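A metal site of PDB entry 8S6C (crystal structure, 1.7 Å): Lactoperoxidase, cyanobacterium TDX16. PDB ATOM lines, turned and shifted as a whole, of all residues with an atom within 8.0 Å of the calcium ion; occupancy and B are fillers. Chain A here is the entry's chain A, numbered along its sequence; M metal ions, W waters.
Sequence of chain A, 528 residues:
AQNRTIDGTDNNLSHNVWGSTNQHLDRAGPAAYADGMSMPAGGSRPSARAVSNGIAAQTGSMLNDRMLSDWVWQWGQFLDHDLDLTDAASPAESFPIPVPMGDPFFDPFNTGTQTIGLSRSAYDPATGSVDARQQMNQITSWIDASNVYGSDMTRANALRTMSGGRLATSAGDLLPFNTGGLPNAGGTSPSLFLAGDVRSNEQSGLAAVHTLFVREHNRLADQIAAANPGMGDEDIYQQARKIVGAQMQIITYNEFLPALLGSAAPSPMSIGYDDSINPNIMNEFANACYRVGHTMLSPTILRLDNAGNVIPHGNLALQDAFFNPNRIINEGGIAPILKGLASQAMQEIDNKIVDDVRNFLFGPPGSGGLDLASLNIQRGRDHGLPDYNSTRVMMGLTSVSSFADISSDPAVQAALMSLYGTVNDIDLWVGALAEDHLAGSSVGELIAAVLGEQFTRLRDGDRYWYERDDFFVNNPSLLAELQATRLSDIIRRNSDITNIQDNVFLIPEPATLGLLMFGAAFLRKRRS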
ATOM      1  N   ALA A  56     -21.324 -22.304  12.800  1.00  0.00           N
ATOM      2  CA  ALA A  56     -19.887 -22.049  12.761  1.00  0.00           C
ATOM      3  C   ALA A  56     -19.479 -21.226  11.541  1.00  0.00           C
ATOM      4  O   ALA A  56     -18.309 -20.839  11.426  1.00  0.00           O
ATOM      5  CB  ALA A  56     -19.113 -23.340  12.790  1.00  0.00           C
ATOM      6  N   GLN A  58     -18.631 -18.299   9.188  1.00  0.00           N
ATOM      7  CA  GLN A  58     -18.160 -16.957   9.450  1.00  0.00           C
ATOM      8  C   GLN A  58     -17.921 -16.222   8.135  1.00  0.00           C
ATOM      9  O   GLN A  58     -17.132 -16.684   7.300  1.00  0.00           O
ATOM     10  CB  GLN A  58     -16.862 -17.121  10.232  1.00  0.00           C
ATOM     11  CG  GLN A  58     -16.303 -15.801  10.753  1.00  0.00           C
ATOM     12  CD  GLN A  58     -15.053 -15.976  11.586  1.00  0.00           C
ATOM     13  OE1 GLN A  58     -14.731 -17.086  12.029  1.00  0.00           O
ATOM     14  NE2 GLN A  58     -14.326 -14.886  11.780  1.00  0.00           N
ATOM     15  N   GLY A  60     -17.053 -12.770   7.972  1.00  0.00           N
ATOM     16  CA  GLY A  60     -16.072 -11.694   8.064  1.00  0.00           C
ATOM     17  C   GLY A  60     -15.141 -11.872   9.257  1.00  0.00           C
ATOM     18  O   GLY A  60     -15.420 -12.706  10.125  1.00  0.00           O
ATOM     19  N   MET A  62     -13.476 -11.297  12.789  1.00  0.00           N
ATOM     20  CA  MET A  62     -14.035 -10.957  14.076  1.00  0.00           C
ATOM     21  C   MET A  62     -12.955 -11.127  15.138  1.00  0.00           C
ATOM     22  O   MET A  62     -12.754 -12.240  15.628  1.00  0.00           O
ATOM     23  CB  MET A  62     -15.236 -11.840  14.418  1.00  0.00           C
ATOM     24  CG  MET A  62     -16.312 -11.814  13.350  1.00  0.00           C
ATOM     25  SD  MET A  62     -17.595 -13.049  13.627  1.00  0.00           S
ATOM     26  CE  MET A  62     -18.020 -12.515  15.297  1.00  0.00           C
ATOM     27  N   LEU A  63     -12.281 -10.016  15.454  1.00  0.00           N
ATOM     28  CA  LEU A  63     -11.188  -9.976  16.403  1.00  0.00           C
ATOM     29  C   LEU A  63     -11.712 -10.178  17.819  1.00  0.00           C
ATOM     30  O   LEU A  63     -12.764  -9.703  18.198  1.00  0.00           O
ATOM     31  CB  LEU A  63     -10.447  -8.647  16.295  1.00  0.00           C
ATOM     32  CG  LEU A  63      -9.743  -8.366  14.972  1.00  0.00           C
ATOM     33  CD1 LEU A  63      -8.989  -7.082  15.162  1.00  0.00           C
ATOM     34  CD2 LEU A  63      -8.831  -9.502  14.505  1.00  0.00           C
ATOM     35  N   ASN A  64     -10.906 -10.891  18.613  1.00  0.00           N
ATOM     36  CA  ASN A  64     -11.205 -11.044  20.029  1.00  0.00           C
ATOM     37  C   ASN A  64     -11.223  -9.668  20.680  1.00  0.00           C
ATOM     38  O   ASN A  64     -10.592  -8.721  20.202  1.00  0.00           O
ATOM     39  CB  ASN A  64     -10.231 -11.977  20.736  1.00  0.00           C
ATOM     40  CG  ASN A  64      -8.918 -11.324  21.095  1.00  0.00           C
ATOM     41  OD1 ASN A  64      -8.727 -10.872  22.243  1.00  0.00           O
ATOM     42  ND2 ASN A  64      -7.993 -11.293  20.149  1.00  0.00           N
ATOM     43  N   VAL A 292     -10.902 -25.182  21.670  1.00  0.00           N
ATOM     44  CA  VAL A 292     -11.326 -23.808  21.476  1.00  0.00           C
ATOM     45  C   VAL A 292     -10.246 -23.085  20.667  1.00  0.00           C
ATOM     46  O   VAL A 292     -10.385 -21.904  20.356  1.00  0.00           O
ATOM     47  CB  VAL A 292     -11.604 -23.268  22.901  1.00  0.00           C
ATOM     48  CG1 VAL A 292     -10.329 -23.119  23.713  1.00  0.00           C
ATOM     49  CG2 VAL A 292     -12.407 -21.980  22.904  1.00  0.00           C
ATOM     50  N   GLY A 293      -9.189 -23.818  20.274  1.00  0.00           N
ATOM     51  CA  GLY A 293      -8.193 -23.320  19.351  1.00  0.00           C
ATOM     52  C   GLY A 293      -8.756 -22.997  17.967  1.00  0.00           C
ATOM     53  O   GLY A 293      -8.411 -21.993  17.366  1.00  0.00           O
ATOM     54  N   HIS A 294      -9.661 -23.841  17.484  1.00  0.00           N
ATOM     55  CA  HIS A 294     -10.125 -23.735  16.112  1.00  0.00           C
ATOM     56  C   HIS A 294     -10.895 -22.424  15.892  1.00  0.00           C
ATOM     57  O   HIS A 294     -10.886 -21.862  14.804  1.00  0.00           O
ATOM     58  CB  HIS A 294     -10.889 -25.027  15.786  1.00  0.00           C
ATOM     59  CG  HIS A 294     -10.081 -26.263  16.106  1.00  0.00           C
ATOM     60  ND1 HIS A 294     -10.645 -27.489  16.375  1.00  0.00           N
ATOM     61  CD2 HIS A 294      -8.736 -26.463  16.142  1.00  0.00           C
ATOM     62  CE1 HIS A 294      -9.675 -28.377  16.630  1.00  0.00           C
ATOM     63  NE2 HIS A 294      -8.492 -27.765  16.623  1.00  0.00           N
ATOM     64  N   THR A 295     -11.550 -21.902  16.942  1.00  0.00           N
ATOM     65  CA  THR A 295     -12.332 -20.683  16.822  1.00  0.00           C
ATOM     66  C   THR A 295     -11.463 -19.427  16.957  1.00  0.00           C
ATOM     67  O   THR A 295     -11.882 -18.336  16.567  1.00  0.00           O
ATOM     68  CB  THR A 295     -13.492 -20.703  17.815  1.00  0.00           C
ATOM     69  OG1 THR A 295     -14.303 -19.571  17.531  1.00  0.00           O
ATOM     70  CG2 THR A 295     -13.049 -20.624  19.267  1.00  0.00           C
ATOM     71  N   MET A 296     -10.241 -19.580  17.488  1.00  0.00           N
ATOM     72  CA  MET A 296      -9.268 -18.508  17.631  1.00  0.00           C
ATOM     73  C   MET A 296      -8.444 -18.273  16.362  1.00  0.00           C
ATOM     74  O   MET A 296      -7.908 -17.168  16.178  1.00  0.00           O
ATOM     75  CB  MET A 296      -8.291 -18.840  18.761  1.00  0.00           C
ATOM     76  CG  MET A 296      -8.928 -19.098  20.118  1.00  0.00           C
ATOM     77  SD  MET A 296      -7.663 -19.442  21.362  1.00  0.00           S
ATOM     78  CE  MET A 296      -8.441 -20.469  22.603  1.00  0.00           C
ATOM     79  N   LEU A 297      -8.359 -19.298  15.496  1.00  0.00           N
ATOM     80  CA  LEU A 297      -7.422 -19.344  14.375  1.00  0.00           C
ATOM     81  C   LEU A 297      -7.633 -18.155  13.430  1.00  0.00           C
ATOM     82  O   LEU A 297      -8.733 -17.874  13.007  1.00  0.00           O
ATOM     83  CB  LEU A 297      -7.543 -20.640  13.567  1.00  0.00           C
ATOM     84  CG  LEU A 297      -7.225 -21.939  14.282  1.00  0.00           C
ATOM     85  CD1 LEU A 297      -7.269 -23.051  13.267  1.00  0.00           C
ATOM     86  CD2 LEU A 297      -5.879 -21.918  14.994  1.00  0.00           C
ATOM     87  N   MET A 346      -5.916 -12.468  17.569  1.00  0.00           N
ATOM     88  CA  MET A 346      -6.615 -13.669  17.180  1.00  0.00           C
ATOM     89  C   MET A 346      -8.109 -13.381  17.030  1.00  0.00           C
ATOM     90  O   MET A 346      -8.638 -12.350  17.468  1.00  0.00           O
ATOM     91  CB  MET A 346      -6.397 -14.784  18.206  1.00  0.00           C
ATOM     92  CG  MET A 346      -7.009 -14.482  19.559  1.00  0.00           C
ATOM     93  SD  MET A 346      -6.801 -15.878  20.690  1.00  0.00           S
ATOM     94  CE  MET A 346      -8.421 -15.836  21.467  1.00  0.00           C
ATOM     95  N   GLN A 347      -8.785 -14.332  16.383  1.00  0.00           N
ATOM     96  CA  GLN A 347     -10.227 -14.286  16.231  1.00  0.00           C
ATOM     97  C   GLN A 347     -10.900 -14.508  17.588  1.00  0.00           C
ATOM     98  O   GLN A 347     -10.349 -15.153  18.477  1.00  0.00           O
ATOM     99  CB  GLN A 347     -10.635 -15.288  15.162  1.00  0.00           C
ATOM    100  CG  GLN A 347     -10.102 -14.964  13.766  1.00  0.00           C
ATOM    101  CD  GLN A 347     -10.714 -13.720  13.148  1.00  0.00           C
ATOM    102  OE1 GLN A 347     -11.916 -13.660  12.861  1.00  0.00           O
ATOM    103  NE2 GLN A 347      -9.898 -12.709  12.944  1.00  0.00           N
ATOM    104  N   GLU A 348     -12.161 -14.074  17.710  1.00  0.00           N
ATOM    105  CA  GLU A 348     -12.897 -14.183  18.956  1.00  0.00           C
ATOM    106  C   GLU A 348     -13.245 -15.655  19.221  1.00  0.00           C
ATOM    107  O   GLU A 348     -13.465 -16.447  18.309  1.00  0.00           O
ATOM    108  CB  GLU A 348     -14.155 -13.315  18.868  1.00  0.00           C
ATOM    109  CG  GLU A 348     -14.929 -13.198  20.183  1.00  0.00           C
ATOM    110  CD  GLU A 348     -14.105 -12.707  21.356  1.00  0.00           C
ATOM    111  OE1 GLU A 348     -13.360 -13.486  22.044  1.00  0.00           O
ATOM    112  OE2 GLU A 348     -14.194 -11.481  21.539  1.00  0.00           O
ATOM    113  N   ILE A 349     -13.363 -15.982  20.499  1.00  0.00           N
ATOM    114  CA  ILE A 349     -13.864 -17.267  20.955  1.00  0.00           C
ATOM    115  C   ILE A 349     -15.410 -17.253  20.935  1.00  0.00           C
ATOM    116  O   ILE A 349     -16.070 -16.497  21.652  1.00  0.00           O
ATOM    117  CB  ILE A 349     -13.302 -17.583  22.351  1.00  0.00           C
ATOM    118  CG1 ILE A 349     -11.785 -17.736  22.244  1.00  0.00           C
ATOM    119  CG2 ILE A 349     -13.963 -18.808  22.987  1.00  0.00           C
ATOM    120  CD1 ILE A 349     -11.064 -18.099  23.525  1.00  0.00           C
ATOM    121  N   ASP A 350     -15.944 -18.100  20.068  1.00  0.00           N
ATOM    122  CA  ASP A 350     -17.352 -18.088  19.709  1.00  0.00           C
ATOM    123  C   ASP A 350     -17.579 -19.303  18.845  1.00  0.00           C
ATOM    124  O   ASP A 350     -16.646 -20.078  18.613  1.00  0.00           O
ATOM    125  CB  ASP A 350     -17.713 -16.775  19.031  1.00  0.00           C
ATOM    126  CG  ASP A 350     -16.899 -16.416  17.804  1.00  0.00           C
ATOM    127  OD1 ASP A 350     -16.359 -17.354  17.141  1.00  0.00           O
ATOM    128  OD2 ASP A 350     -16.879 -15.218  17.488  1.00  0.00           O
ATOM    129  N   ASN A 351     -18.790 -19.446  18.290  1.00  0.00           N
ATOM    130  CA  ASN A 351     -19.065 -20.618  17.470  1.00  0.00           C
ATOM    131  C   ASN A 351     -18.371 -20.515  16.102  1.00  0.00           C
ATOM    132  O   ASN A 351     -18.270 -21.502  15.379  1.00  0.00           O
ATOM    133  CB  ASN A 351     -20.578 -20.806  17.283  1.00  0.00           C
ATOM    134  CG  ASN A 351     -21.253 -21.315  18.536  1.00  0.00           C
ATOM    135  OD1 ASN A 351     -21.922 -20.568  19.241  1.00  0.00           O
ATOM    136  ND2 ASN A 351     -21.018 -22.578  18.863  1.00  0.00           N
ATOM    137  N   LYS A 352     -17.990 -19.297  15.707  1.00  0.00           N
ATOM    138  CA  LYS A 352     -17.546 -19.038  14.342  1.00  0.00           C
ATOM    139  C   LYS A 352     -16.103 -19.476  14.115  1.00  0.00           C
ATOM    140  O   LYS A 352     -15.233 -19.104  14.893  1.00  0.00           O
ATOM    141  CB  LYS A 352     -17.719 -17.549  14.029  1.00  0.00           C
ATOM    142  CG  LYS A 352     -19.171 -17.154  13.862  1.00  0.00           C
ATOM    143  CD  LYS A 352     -19.432 -15.672  13.676  1.00  0.00           C
ATOM    144  CE  LYS A 352     -20.798 -15.389  13.115  1.00  0.00           C
ATOM    145  NZ  LYS A 352     -21.823 -16.280  13.682  1.00  0.00           N
ATOM    146  N   ILE A 353     -15.885 -20.232  13.031  1.00  0.00           N
ATOM    147  CA  ILE A 353     -14.595 -20.742  12.578  1.00  0.00           C
ATOM    148  C   ILE A 353     -14.340 -20.161  11.181  1.00  0.00           C
ATOM    149  O   ILE A 353     -15.223 -20.227  10.348  1.00  0.00           O
ATOM    150  CB  ILE A 353     -14.631 -22.288  12.496  1.00  0.00           C
ATOM    151  CG1 ILE A 353     -15.204 -22.913  13.776  1.00  0.00           C
ATOM    152  CG2 ILE A 353     -13.290 -22.905  12.126  1.00  0.00           C
ATOM    153  CD1 ILE A 353     -14.428 -22.552  15.011  1.00  0.00           C
ATOM    154  N   VAL A 354     -13.128 -19.681  10.902  1.00  0.00           N
ATOM    155  CA  VAL A 354     -12.824 -19.080   9.621  1.00  0.00           C
ATOM    156  C   VAL A 354     -12.951 -20.130   8.514  1.00  0.00           C
ATOM    157  O   VAL A 354     -12.760 -21.323   8.746  1.00  0.00           O
ATOM    158  CB  VAL A 354     -11.431 -18.394   9.590  1.00  0.00           C
ATOM    159  CG1 VAL A 354     -11.355 -17.239  10.583  1.00  0.00           C
ATOM    160  CG2 VAL A 354     -10.282 -19.378   9.810  1.00  0.00           C
ATOM    161  N   LEU A 433     -18.851 -23.305  23.243  1.00  0.00           N
ATOM    162  CA  LEU A 433     -18.425 -22.135  22.503  1.00  0.00           C
ATOM    163  C   LEU A 433     -19.532 -21.100  22.356  1.00  0.00           C
ATOM    164  O   LEU A 433     -19.242 -19.999  21.948  1.00  0.00           O
ATOM    165  CB  LEU A 433     -17.889 -22.527  21.122  1.00  0.00           C
ATOM    166  CG  LEU A 433     -16.485 -23.132  21.103  1.00  0.00           C
ATOM    167  CD1 LEU A 433     -16.113 -23.517  19.670  1.00  0.00           C
ATOM    168  CD2 LEU A 433     -15.472 -22.198  21.674  1.00  0.00           C
HETATM  169 CA    CA M   1     -14.127 -17.535  16.251  1.00  0.00          CA
HETATM  170  O   HOH W   1     -13.011 -17.351  14.135  1.00  0.00           O
HETATM  171  O   HOH W   2     -14.843 -15.407  15.512  1.00  0.00           O
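The calcium ion is bound by the backbone carbonyl oxygen of Lys 352 (2.4 Å), water W2 (2.4 Å), water W1 (2.4 Å), the backbone carbonyl oxygen of Thr 295 (2.4 Å), the side-chain carboxylate of Asp 350 (2.4 Å), the side-chain hydroxyl of Thr 295 (2.4 Å) and the backbone carbonyl oxygen of Glu 348 (2.4 Å).
N of Glu 348 sits at hydrogen-bond distance from O of Met 62, 2.8 Å away.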
